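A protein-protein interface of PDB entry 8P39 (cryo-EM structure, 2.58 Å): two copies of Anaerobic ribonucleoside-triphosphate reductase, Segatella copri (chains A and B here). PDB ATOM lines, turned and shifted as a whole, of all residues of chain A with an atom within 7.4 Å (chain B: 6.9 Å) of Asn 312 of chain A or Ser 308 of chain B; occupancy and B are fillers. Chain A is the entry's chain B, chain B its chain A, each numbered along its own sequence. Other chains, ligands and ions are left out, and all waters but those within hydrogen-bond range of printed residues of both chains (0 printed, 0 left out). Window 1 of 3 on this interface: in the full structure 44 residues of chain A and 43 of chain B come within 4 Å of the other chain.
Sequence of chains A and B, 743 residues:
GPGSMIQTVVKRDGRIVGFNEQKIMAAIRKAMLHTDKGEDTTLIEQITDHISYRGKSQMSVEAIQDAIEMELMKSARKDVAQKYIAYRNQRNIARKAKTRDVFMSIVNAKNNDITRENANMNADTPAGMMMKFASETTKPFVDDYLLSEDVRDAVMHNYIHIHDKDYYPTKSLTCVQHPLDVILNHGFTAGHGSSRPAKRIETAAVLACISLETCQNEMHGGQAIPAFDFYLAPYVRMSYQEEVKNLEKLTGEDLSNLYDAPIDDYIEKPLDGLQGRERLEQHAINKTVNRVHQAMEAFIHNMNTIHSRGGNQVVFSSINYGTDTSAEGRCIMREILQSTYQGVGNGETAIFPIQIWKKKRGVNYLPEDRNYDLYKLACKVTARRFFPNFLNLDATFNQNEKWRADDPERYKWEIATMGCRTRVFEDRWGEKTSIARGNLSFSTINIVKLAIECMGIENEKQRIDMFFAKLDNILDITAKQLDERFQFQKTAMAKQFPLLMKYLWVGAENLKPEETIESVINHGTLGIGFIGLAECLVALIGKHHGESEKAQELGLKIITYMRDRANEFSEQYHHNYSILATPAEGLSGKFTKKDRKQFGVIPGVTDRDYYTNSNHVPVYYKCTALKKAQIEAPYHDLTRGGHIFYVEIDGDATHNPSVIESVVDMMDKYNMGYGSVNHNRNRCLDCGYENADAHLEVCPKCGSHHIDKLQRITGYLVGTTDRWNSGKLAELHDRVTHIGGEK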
ATOM      1  N   MET A 121      -3.349   5.521  -0.096  1.00  0.00           N
ATOM      2  CA  MET A 121      -3.411   5.246   1.330  1.00  0.00           C
ATOM      3  C   MET A 121      -2.190   5.821   2.034  1.00  0.00           C
ATOM      4  O   MET A 121      -1.110   5.940   1.448  1.00  0.00           O
ATOM      5  CB  MET A 121      -3.504   3.741   1.597  1.00  0.00           C
ATOM      6  CG  MET A 121      -4.673   3.061   0.909  1.00  0.00           C
ATOM      7  SD  MET A 121      -4.894   1.354   1.445  1.00  0.00           S
ATOM      8  CE  MET A 121      -3.278   0.671   1.083  1.00  0.00           C
ATOM      9  N   ALA A 127      -5.326   4.521  10.828  1.00  0.00           N
ATOM     10  CA  ALA A 127      -6.257   3.985   9.840  1.00  0.00           C
ATOM     11  C   ALA A 127      -5.526   3.166   8.785  1.00  0.00           C
ATOM     12  O   ALA A 127      -6.006   2.107   8.365  1.00  0.00           O
ATOM     13  CB  ALA A 127      -7.046   5.120   9.192  1.00  0.00           C
ATOM     14  N   MET A 131      -5.614  -1.261   8.014  1.00  0.00           N
ATOM     15  CA  MET A 131      -5.861  -1.832   6.692  1.00  0.00           C
ATOM     16  C   MET A 131      -4.749  -2.793   6.286  1.00  0.00           C
ATOM     17  O   MET A 131      -5.015  -3.848   5.701  1.00  0.00           O
ATOM     18  CB  MET A 131      -6.014  -0.716   5.657  1.00  0.00           C
ATOM     19  CG  MET A 131      -7.274   0.129   5.816  1.00  0.00           C
ATOM     20  SD  MET A 131      -8.801  -0.759   5.437  1.00  0.00           S
ATOM     21  CE  MET A 131      -9.398  -1.157   7.078  1.00  0.00           C
ATOM     22  N   TYR A 167      -9.901  -7.595  -0.949  1.00  0.00           N
ATOM     23  CA  TYR A 167     -11.345  -7.492  -0.807  1.00  0.00           C
ATOM     24  C   TYR A 167     -12.079  -8.696  -1.374  1.00  0.00           C
ATOM     25  O   TYR A 167     -13.301  -8.636  -1.539  1.00  0.00           O
ATOM     26  CB  TYR A 167     -11.849  -6.213  -1.478  1.00  0.00           C
ATOM     27  CG  TYR A 167     -11.655  -4.968  -0.644  1.00  0.00           C
ATOM     28  CD1 TYR A 167     -10.483  -4.230  -0.727  1.00  0.00           C
ATOM     29  CD2 TYR A 167     -12.647  -4.531   0.225  1.00  0.00           C
ATOM     30  CE1 TYR A 167     -10.304  -3.093   0.033  1.00  0.00           C
ATOM     31  CE2 TYR A 167     -12.476  -3.397   0.988  1.00  0.00           C
ATOM     32  CZ  TYR A 167     -11.303  -2.682   0.888  1.00  0.00           C
ATOM     33  OH  TYR A 167     -11.127  -1.549   1.645  1.00  0.00           O
ATOM     34  N   GLU A 213     -19.204  10.013  -1.082  1.00  0.00           N
ATOM     35  CA  GLU A 213     -18.547   9.519   0.126  1.00  0.00           C
ATOM     36  C   GLU A 213     -19.221   8.254   0.641  1.00  0.00           C
ATOM     37  O   GLU A 213     -18.550   7.296   1.042  1.00  0.00           O
ATOM     38  CB  GLU A 213     -18.553  10.603   1.203  1.00  0.00           C
ATOM     39  CG  GLU A 213     -17.184  11.150   1.559  1.00  0.00           C
ATOM     40  CD  GLU A 213     -16.362  10.190   2.401  1.00  0.00           C
ATOM     41  OE1 GLU A 213     -16.907   9.155   2.836  1.00  0.00           O
ATOM     42  OE2 GLU A 213     -15.168  10.477   2.629  1.00  0.00           O
ATOM     43  N   GLN A 216     -18.588   5.070  -1.613  1.00  0.00           N
ATOM     44  CA  GLN A 216     -17.212   4.585  -1.645  1.00  0.00           C
ATOM     45  C   GLN A 216     -16.991   3.474  -0.630  1.00  0.00           C
ATOM     46  O   GLN A 216     -16.307   2.486  -0.918  1.00  0.00           O
ATOM     47  CB  GLN A 216     -16.237   5.732  -1.392  1.00  0.00           C
ATOM     48  CG  GLN A 216     -14.786   5.294  -1.353  1.00  0.00           C
ATOM     49  CD  GLN A 216     -14.306   4.739  -2.678  1.00  0.00           C
ATOM     50  OE1 GLN A 216     -13.841   5.481  -3.541  1.00  0.00           O
ATOM     51  NE2 GLN A 216     -14.412   3.427  -2.846  1.00  0.00           N
ATOM     52  N   ASN A 217     -17.563   3.612   0.559  1.00  0.00           N
ATOM     53  CA  ASN A 217     -17.397   2.613   1.608  1.00  0.00           C
ATOM     54  C   ASN A 217     -18.099   1.305   1.297  1.00  0.00           C
ATOM     55  O   ASN A 217     -18.102   0.413   2.153  1.00  0.00           O
ATOM     56  CB  ASN A 217     -17.899   3.168   2.942  1.00  0.00           C
ATOM     57  CG  ASN A 217     -17.155   4.416   3.370  1.00  0.00           C
ATOM     58  OD1 ASN A 217     -16.050   4.686   2.900  1.00  0.00           O
ATOM     59  ND2 ASN A 217     -17.757   5.184   4.268  1.00  0.00           N
ATOM     60  N   GLU A 218     -18.693   1.154   0.113  1.00  0.00           N
ATOM     61  CA  GLU A 218     -19.334  -0.090  -0.280  1.00  0.00           C
ATOM     62  C   GLU A 218     -18.688  -0.739  -1.496  1.00  0.00           C
ATOM     63  O   GLU A 218     -19.161  -1.790  -1.939  1.00  0.00           O
ATOM     64  CB  GLU A 218     -20.826   0.144  -0.558  1.00  0.00           C
ATOM     65  CG  GLU A 218     -21.510   1.097   0.415  1.00  0.00           C
ATOM     66  CD  GLU A 218     -21.469   0.614   1.855  1.00  0.00           C
ATOM     67  OE1 GLU A 218     -21.357  -0.609   2.078  1.00  0.00           O
ATOM     68  OE2 GLU A 218     -21.550   1.464   2.766  1.00  0.00           O
ATOM     69  N   ILE A 306     -11.883  15.033   1.746  1.00  0.00           N
ATOM     70  CA  ILE A 306     -12.248  13.689   2.182  1.00  0.00           C
ATOM     71  C   ILE A 306     -11.202  12.670   1.747  1.00  0.00           C
ATOM     72  O   ILE A 306     -10.942  11.697   2.463  1.00  0.00           O
ATOM     73  CB  ILE A 306     -13.648  13.316   1.663  1.00  0.00           C
ATOM     74  CG1 ILE A 306     -13.714  13.476   0.143  1.00  0.00           C
ATOM     75  CG2 ILE A 306     -14.710  14.168   2.340  1.00  0.00           C
ATOM     76  CD1 ILE A 306     -15.034  13.074  -0.465  1.00  0.00           C
ATOM     77  N   ARG A 309      -8.143  12.187   4.029  1.00  0.00           N
ATOM     78  CA  ARG A 309      -8.365  11.411   5.243  1.00  0.00           C
ATOM     79  C   ARG A 309      -9.162  10.156   4.915  1.00  0.00           C
ATOM     80  O   ARG A 309      -9.366   9.834   3.740  1.00  0.00           O
ATOM     81  CB  ARG A 309      -9.088  12.252   6.296  1.00  0.00           C
ATOM     82  CG  ARG A 309     -10.465  12.732   5.872  1.00  0.00           C
ATOM     83  CD  ARG A 309     -11.539  12.227   6.818  1.00  0.00           C
ATOM     84  NE  ARG A 309     -12.862  12.730   6.469  1.00  0.00           N
ATOM     85  CZ  ARG A 309     -13.746  12.074   5.731  1.00  0.00           C
ATOM     86  NH1 ARG A 309     -13.484  10.872   5.244  1.00  0.00           N
ATOM     87  NH2 ARG A 309     -14.924  12.636   5.478  1.00  0.00           N
ATOM     88  N   GLY A 310      -9.600   9.432   5.939  1.00  0.00           N
ATOM     89  CA  GLY A 310     -10.449   8.279   5.727  1.00  0.00           C
ATOM     90  C   GLY A 310      -9.946   7.013   6.387  1.00  0.00           C
ATOM     91  O   GLY A 310      -8.820   6.577   6.136  1.00  0.00           O
ATOM     92  N   GLY A 311     -10.777   6.417   7.238  1.00  0.00           N
ATOM     93  CA  GLY A 311     -10.446   5.149   7.854  1.00  0.00           C
ATOM     94  C   GLY A 311     -10.903   3.983   7.005  1.00  0.00           C
ATOM     95  O   GLY A 311     -10.388   2.867   7.128  1.00  0.00           O
ATOM     96  N   ASN A 312     -11.876   4.237   6.138  1.00  0.00           N
ATOM     97  CA  ASN A 312     -12.369   3.241   5.202  1.00  0.00           C
ATOM     98  C   ASN A 312     -11.581   3.351   3.898  1.00  0.00           C
ATOM     99  O   ASN A 312     -10.534   4.001   3.834  1.00  0.00           O
ATOM    100  CB  ASN A 312     -13.870   3.417   4.988  1.00  0.00           C
ATOM    101  CG  ASN A 312     -14.623   3.591   6.289  1.00  0.00           C
ATOM    102  OD1 ASN A 312     -14.049   3.990   7.302  1.00  0.00           O
ATOM    103  ND2 ASN A 312     -15.917   3.295   6.270  1.00  0.00           N
ATOM    104  N   GLN A 313     -12.066   2.694   2.847  1.00  0.00           N
ATOM    105  CA  GLN A 313     -11.419   2.788   1.547  1.00  0.00           C
ATOM    106  C   GLN A 313     -11.414   4.233   1.064  1.00  0.00           C
ATOM    107  O   GLN A 313     -12.402   4.958   1.208  1.00  0.00           O
ATOM    108  CB  GLN A 313     -12.131   1.890   0.536  1.00  0.00           C
ATOM    109  CG  GLN A 313     -11.369   1.675  -0.763  1.00  0.00           C
ATOM    110  CD  GLN A 313     -10.178   0.747  -0.602  1.00  0.00           C
ATOM    111  OE1 GLN A 313      -9.990   0.132   0.447  1.00  0.00           O
ATOM    112  NE2 GLN A 313      -9.369   0.639  -1.649  1.00  0.00           N
ATOM    113  N   VAL A 314     -10.284   4.653   0.493  1.00  0.00           N
ATOM    114  CA  VAL A 314     -10.121   6.039   0.075  1.00  0.00           C
ATOM    115  C   VAL A 314     -11.109   6.366  -1.041  1.00  0.00           C
ATOM    116  O   VAL A 314     -11.479   5.506  -1.851  1.00  0.00           O
ATOM    117  CB  VAL A 314      -8.668   6.297  -0.365  1.00  0.00           C
ATOM    118  CG1 VAL A 314      -8.364   7.783  -0.356  1.00  0.00           C
ATOM    119  CG2 VAL A 314      -7.705   5.551   0.542  1.00  0.00           C
ATOM    120  N   VAL A 315     -11.538   7.625  -1.087  1.00  0.00           N
ATOM    121  CA  VAL A 315     -12.622   8.053  -1.966  1.00  0.00           C
ATOM    122  C   VAL A 315     -12.060   8.364  -3.347  1.00  0.00           C
ATOM    123  O   VAL A 315     -11.153   9.190  -3.488  1.00  0.00           O
ATOM    124  CB  VAL A 315     -13.359   9.270  -1.387  1.00  0.00           C
ATOM    125  CG1 VAL A 315     -14.604   9.569  -2.205  1.00  0.00           C
ATOM    126  CG2 VAL A 315     -13.719   9.025   0.069  1.00  0.00           C
ATOM    127  N   THR B 125     -20.974  -4.206   6.346  1.00  0.00           N
ATOM    128  CA  THR B 125     -20.479  -3.479   5.193  1.00  0.00           C
ATOM    129  C   THR B 125     -19.046  -3.904   4.880  1.00  0.00           C
ATOM    130  O   THR B 125     -18.312  -4.340   5.771  1.00  0.00           O
ATOM    131  CB  THR B 125     -20.536  -1.975   5.451  1.00  0.00           C
ATOM    132  OG1 THR B 125     -19.682  -1.289   4.527  1.00  0.00           O
ATOM    133  CG2 THR B 125     -20.099  -1.660   6.872  1.00  0.00           C
ATOM    134  N   ALA B 127     -16.439  -2.105   4.362  1.00  0.00           N
ATOM    135  CA  ALA B 127     -15.520  -1.358   5.215  1.00  0.00           C
ATOM    136  C   ALA B 127     -15.604  -1.830   6.663  1.00  0.00           C
ATOM    137  O   ALA B 127     -14.591  -1.865   7.371  1.00  0.00           O
ATOM    138  CB  ALA B 127     -15.812   0.138   5.119  1.00  0.00           C
ATOM    139  N   GLY B 128     -16.804  -2.184   7.122  1.00  0.00           N
ATOM    140  CA  GLY B 128     -16.954  -2.658   8.489  1.00  0.00           C
ATOM    141  C   GLY B 128     -16.319  -4.016   8.728  1.00  0.00           C
ATOM    142  O   GLY B 128     -15.676  -4.235   9.757  1.00  0.00           O
ATOM    143  N   GLU B 213     -14.035  15.397  11.911  1.00  0.00           N
ATOM    144  CA  GLU B 213     -13.983  14.201  11.078  1.00  0.00           C
ATOM    145  C   GLU B 213     -12.570  13.698  10.825  1.00  0.00           C
ATOM    146  O   GLU B 213     -12.360  12.483  10.765  1.00  0.00           O
ATOM    147  CB  GLU B 213     -14.662  14.466   9.729  1.00  0.00           C
ATOM    148  CG  GLU B 213     -16.146  14.777   9.820  1.00  0.00           C
ATOM    149  CD  GLU B 213     -16.979  13.559  10.155  1.00  0.00           C
ATOM    150  OE1 GLU B 213     -16.509  12.431   9.904  1.00  0.00           O
ATOM    151  OE2 GLU B 213     -18.105  13.730  10.666  1.00  0.00           O
ATOM    152  N   THR B 214     -11.599  14.600  10.676  1.00  0.00           N
ATOM    153  CA  THR B 214     -10.230  14.175  10.409  1.00  0.00           C
ATOM    154  C   THR B 214      -9.567  13.607  11.659  1.00  0.00           C
ATOM    155  O   THR B 214      -8.840  12.610  11.585  1.00  0.00           O
ATOM    156  CB  THR B 214      -9.421  15.349   9.859  1.00  0.00           C
ATOM    157  OG1 THR B 214     -10.076  15.879   8.701  1.00  0.00           O
ATOM    158  CG2 THR B 214      -8.020  14.903   9.478  1.00  0.00           C
ATOM    159  N   GLN B 216     -10.883  12.063  14.153  1.00  0.00           N
ATOM    160  CA  GLN B 216     -11.445  10.805  14.629  1.00  0.00           C
ATOM    161  C   GLN B 216     -10.660   9.611  14.104  1.00  0.00           C
ATOM    162  O   GLN B 216     -10.440   8.634  14.831  1.00  0.00           O
ATOM    163  CB  GLN B 216     -12.914  10.701  14.226  1.00  0.00           C
ATOM    164  CG  GLN B 216     -13.595   9.453  14.735  1.00  0.00           C
ATOM    165  CD  GLN B 216     -13.488   9.309  16.238  1.00  0.00           C
ATOM    166  OE1 GLN B 216     -13.800  10.237  16.985  1.00  0.00           O
ATOM    167  NE2 GLN B 216     -13.037   8.146  16.692  1.00  0.00           N
ATOM    168  N   ASN B 217     -10.225   9.669  12.844  1.00  0.00           N
ATOM    169  CA  ASN B 217      -9.449   8.580  12.263  1.00  0.00           C
ATOM    170  C   ASN B 217      -8.062   8.449  12.879  1.00  0.00           C
ATOM    171  O   ASN B 217      -7.389   7.444  12.636  1.00  0.00           O
ATOM    172  CB  ASN B 217      -9.325   8.775  10.751  1.00  0.00           C
ATOM    173  CG  ASN B 217     -10.662   8.699  10.046  1.00  0.00           C
ATOM    174  OD1 ASN B 217     -11.573   8.003  10.491  1.00  0.00           O
ATOM    175  ND2 ASN B 217     -10.786   9.414   8.936  1.00  0.00           N
ATOM    176  N   THR B 305     -25.245  12.533   9.486  1.00  0.00           N
ATOM    177  CA  THR B 305     -25.404  11.700   8.303  1.00  0.00           C
ATOM    178  C   THR B 305     -24.098  11.309   7.625  1.00  0.00           C
ATOM    179  O   THR B 305     -24.127  10.476   6.712  1.00  0.00           O
ATOM    180  CB  THR B 305     -26.300  12.398   7.267  1.00  0.00           C
ATOM    181  OG1 THR B 305     -26.770  11.437   6.315  1.00  0.00           O
ATOM    182  CG2 THR B 305     -25.524  13.479   6.531  1.00  0.00           C
ATOM    183  N   ILE B 306     -22.964  11.869   8.032  1.00  0.00           N
ATOM    184  CA  ILE B 306     -21.679  11.547   7.421  1.00  0.00           C
ATOM    185  C   ILE B 306     -21.060  10.385   8.191  1.00  0.00           C
ATOM    186  O   ILE B 306     -20.643  10.540   9.342  1.00  0.00           O
ATOM    187  CB  ILE B 306     -20.744  12.763   7.398  1.00  0.00           C
ATOM    188  CG1 ILE B 306     -21.310  13.849   6.484  1.00  0.00           C
ATOM    189  CG2 ILE B 306     -19.355  12.358   6.938  1.00  0.00           C
ATOM    190  CD1 ILE B 306     -21.473  13.414   5.046  1.00  0.00           C
ATOM    191  N   HIS B 307     -21.004   9.217   7.555  1.00  0.00           N
ATOM    192  CA  HIS B 307     -20.379   8.032   8.134  1.00  0.00           C
ATOM    193  C   HIS B 307     -18.950   7.948   7.613  1.00  0.00           C
ATOM    194  O   HIS B 307     -18.728   7.631   6.440  1.00  0.00           O
ATOM    195  CB  HIS B 307     -21.169   6.777   7.777  1.00  0.00           C
ATOM    196  CG  HIS B 307     -22.639   6.894   8.033  1.00  0.00           C
ATOM    197  ND1 HIS B 307     -23.236   6.414   9.179  1.00  0.00           N
ATOM    198  CD2 HIS B 307     -23.633   7.431   7.289  1.00  0.00           C
ATOM    199  CE1 HIS B 307     -24.534   6.654   9.130  1.00  0.00           C
ATOM    200  NE2 HIS B 307     -24.801   7.270   7.993  1.00  0.00           N
ATOM    201  N   SER B 308     -17.978   8.230   8.478  1.00  0.00           N
ATOM    202  CA  SER B 308     -16.595   8.329   8.032  1.00  0.00           C
ATOM    203  C   SER B 308     -15.657   7.446   8.848  1.00  0.00           C
ATOM    204  O   SER B 308     -14.634   6.983   8.333  1.00  0.00           O
ATOM    205  CB  SER B 308     -16.126   9.784   8.091  1.00  0.00           C
ATOM    206  OG  SER B 308     -14.775   9.899   7.682  1.00  0.00           O
ATOM    207  N   ARG B 309     -15.988   7.212  10.115  1.00  0.00           N
ATOM    208  CA  ARG B 309     -15.137   6.396  10.968  1.00  0.00           C
ATOM    209  C   ARG B 309     -15.118   4.948  10.484  1.00  0.00           C
ATOM    210  O   ARG B 309     -16.093   4.444   9.924  1.00  0.00           O
ATOM    211  CB  ARG B 309     -15.615   6.467  12.422  1.00  0.00           C
ATOM    212  CG  ARG B 309     -14.808   5.620  13.398  1.00  0.00           C
ATOM    213  CD  ARG B 309     -14.891   6.149  14.819  1.00  0.00           C
ATOM    214  NE  ARG B 309     -16.240   6.093  15.368  1.00  0.00           N
ATOM    215  CZ  ARG B 309     -16.695   5.115  16.137  1.00  0.00           C
ATOM    216  NH1 ARG B 309     -15.937   4.080  16.460  1.00  0.00           N
ATOM    217  NH2 ARG B 309     -17.940   5.179  16.599  1.00  0.00           N
ATOM    218  N   GLY B 310     -13.982   4.285  10.685  1.00  0.00           N
ATOM    219  CA  GLY B 310     -13.880   2.877  10.345  1.00  0.00           C
ATOM    220  C   GLY B 310     -14.568   2.010  11.388  1.00  0.00           C
ATOM    221  O   GLY B 310     -14.406   2.201  12.594  1.00  0.00           O
ATOM    222  N   GLY B 311     -15.345   1.045  10.907  1.00  0.00           N
ATOM    223  CA  GLY B 311     -16.057   0.149  11.797  1.00  0.00           C
ATOM    224  C   GLY B 311     -17.453   0.625  12.146  1.00  0.00           C
ATOM    225  O   GLY B 311     -18.398   0.408  11.383  1.00  0.00           O
ATOM    226  N   GLN B 313     -18.618   3.478  12.060  1.00  0.00           N
ATOM    227  CA  GLN B 313     -19.010   4.429  11.024  1.00  0.00           C
ATOM    228  C   GLN B 313     -19.819   5.603  11.558  1.00  0.00           C
ATOM    229  O   GLN B 313     -20.685   6.129  10.852  1.00  0.00           O
ATOM    230  CB  GLN B 313     -19.782   3.736   9.894  1.00  0.00           C
ATOM    231  CG  GLN B 313     -18.904   2.962   8.922  1.00  0.00           C
ATOM    232  CD  GLN B 313     -19.701   2.317   7.806  1.00  0.00           C
ATOM    233  OE1 GLN B 313     -19.455   2.566   6.627  1.00  0.00           O
ATOM    234  NE2 GLN B 313     -20.662   1.480   8.175  1.00  0.00           N
ATOM    235  N   VAL B 314     -19.568   6.029  12.792  1.00  0.00           N
ATOM    236  CA  VAL B 314     -20.185   7.226  13.350  1.00  0.00           C
ATOM    237  C   VAL B 314     -19.119   8.001  14.112  1.00  0.00           C
ATOM    238  O   VAL B 314     -18.322   7.410  14.849  1.00  0.00           O
ATOM    239  CB  VAL B 314     -21.386   6.888  14.257  1.00  0.00           C
ATOM    240  CG1 VAL B 314     -20.986   5.908  15.351  1.00  0.00           C
ATOM    241  CG2 VAL B 314     -21.978   8.155  14.852  1.00  0.00           C
ATOM    242  N   VAL B 315     -19.089   9.315  13.916  1.00  0.00           N
ATOM    243  CA  VAL B 315     -18.133  10.181  14.595  1.00  0.00           C
ATOM    244  C   VAL B 315     -18.808  10.788  15.818  1.00  0.00           C
ATOM    245  O   VAL B 315     -19.840  11.456  15.699  1.00  0.00           O
ATOM    246  CB  VAL B 315     -17.608  11.274  13.655  1.00  0.00           C
ATOM    247  CG1 VAL B 315     -16.823  12.307  14.438  1.00  0.00           C
ATOM    248  CG2 VAL B 315     -16.749  10.661  12.567  1.00  0.00           C
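N of Ala 127 of chain B touches O of Asn 217 of chain A, 3.7 Å away. Asn 217 of chain A touches Gln 313 of chain B. Arg 309 of chain A touches Asn 217 of chain B. Asn 312 of chain A touches Ala 127 of chain B (ND2 to CB, 3.4 Å). Asn 312 of chain A touches Gln 313 of chain B.
Of chain B, only Asn 217 comes within 4 Å of Gly 311 of chain A. Of chain B, only Ala 127 (3.4 Å), Ser 308 (3.2 Å), Arg 309 (3.4 Å), Gly 310 (3.2 Å) and Gln 313 (3.6 Å) come within 4 Å of Asn 312 of chain A. Val 314 of chain A touches none of the printed residues of chain B. Of the printed residues of chain A, Ala 127 of chain B touches Asn 217 and Asn 312. Thr 305 of chain B touches none of the printed residues of chain A. Of the printed residues of chain A, His 307 of chain B touches Asn 217 (3.4 Å). Ser 308 of chain B touches just these residues of chain A: Arg 309 (2.9 Å) and Asn 312 (3.2 Å). The nearest printed residue of chain B that does not touch Arg 309 of chain A is Glu 213 of chain B (4.04 Å).
Of the 16 printed residues of chain A, 6 touch a printed residue of chain B. Printed residues of chain A that touch a printed residue of chain B: Asn 217, Glu 218, Arg 309, Gly 310, Gly 311 and Asn 312. Along chain A the printed residues that touch a printed residue of chain B span positions 217 to 312. Of the 17 printed residues of chain B, 8 touch a printed residue of chain A. Hydrophobic or aromatic side chains of chain B within 4 Å of the printed part of chain A: Ala 127. Among the printed residues, 14 pairs touch across the chains. Among the printed residues, no Asp or Glu carboxylate lies within 4 Å of a Lys or Arg side-chain nitrogen of the other chain.
Asn 217 of chain A touches Ala 127 of chain B, but with the chains exchanged Ala 127 of chain A does not touch Asn 217 of chain B (4.01 Å). Asn 217 of chain A touches Gln 313 of chain B, but with the chains exchanged Gln 313 of chain A does not touch Asn 217 of chain B (9.1 Å). Gly 310 of chain A touches Asn 217 of chain B, but with the chains exchanged Asn 217 of chain A does not touch Gly 310 of chain B (7.5 Å). Gly 311 of chain A touches Asn 217 of chain B, but with the chains exchanged Asn 217 of chain A does not touch Gly 311 of chain B (8.2 Å). Positions printed for both chains: 127, 213, 216, 217, 306, 309, 310, 311, 313, 314 and 315.
The side-chain hydroxyl of Thr 125 of chain B is in hydrogen-bond range of the backbone carbonyl oxygen of Asn 217 of chain A, 3.3 Å away. The side-chain hydroxyl (OG1) of Thr 125 of chain B lies within hydrogen-bond range of the side-chain carboxylate (OE1) of Glu 218 of chain A (3.0 Å). N of Gly 310 of chain A lies close to ND2 of Asn 217 of chain B (3.2 Å). The side-chain amide nitrogen (ND2) of Asn 217 of chain B sits close to the backbone NH (N) of Gly 311 of chain A, at 3.4 Å. The side-chain amide nitrogen (ND2) of Asn 217 of chain A lies within hydrogen-bond range of the backbone carbonyl oxygen (O) of His 307 of chain B, at 3.4 Å. The guanidinium group (NH1) of Arg 309 of chain A is in hydrogen-bond range of the side-chain hydroxyl (OG) of Ser 308 of chain B (2.9 Å). O of Ser 308 of chain B sits close to OD1 of Asn 312 of chain A, 3.2 Å away. O of Arg 309 of chain B sits close to OD1 of Asn 312 of chain A (3.4 Å). N of Gly 310 of chain B lies close to OD1 of Asn 312 of chain A (3.4 Å).
The side-chain hydroxyl (OG1) of Thr 125 of chain B sits close to the backbone NH (N) of Ala 127 of chain B (3.3 Å). O of Gln 313 of chain B sits at hydrogen-bond distance from ND1 of His 307 of chain B, at 3.1 Å. O of Val 314 of chain B lies within hydrogen-bond range of NE of Arg 309 of chain B. NH1 of Arg 309 of chain A lies within salt-bridge range of OE2 of Glu 213 of chain A (3.1 Å). The side-chain amide nitrogen (ND2) of Asn 312 of chain A lies close to the side-chain amide nitrogen (ND2) of Asn 217 of chain A, 3.3 Å away.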
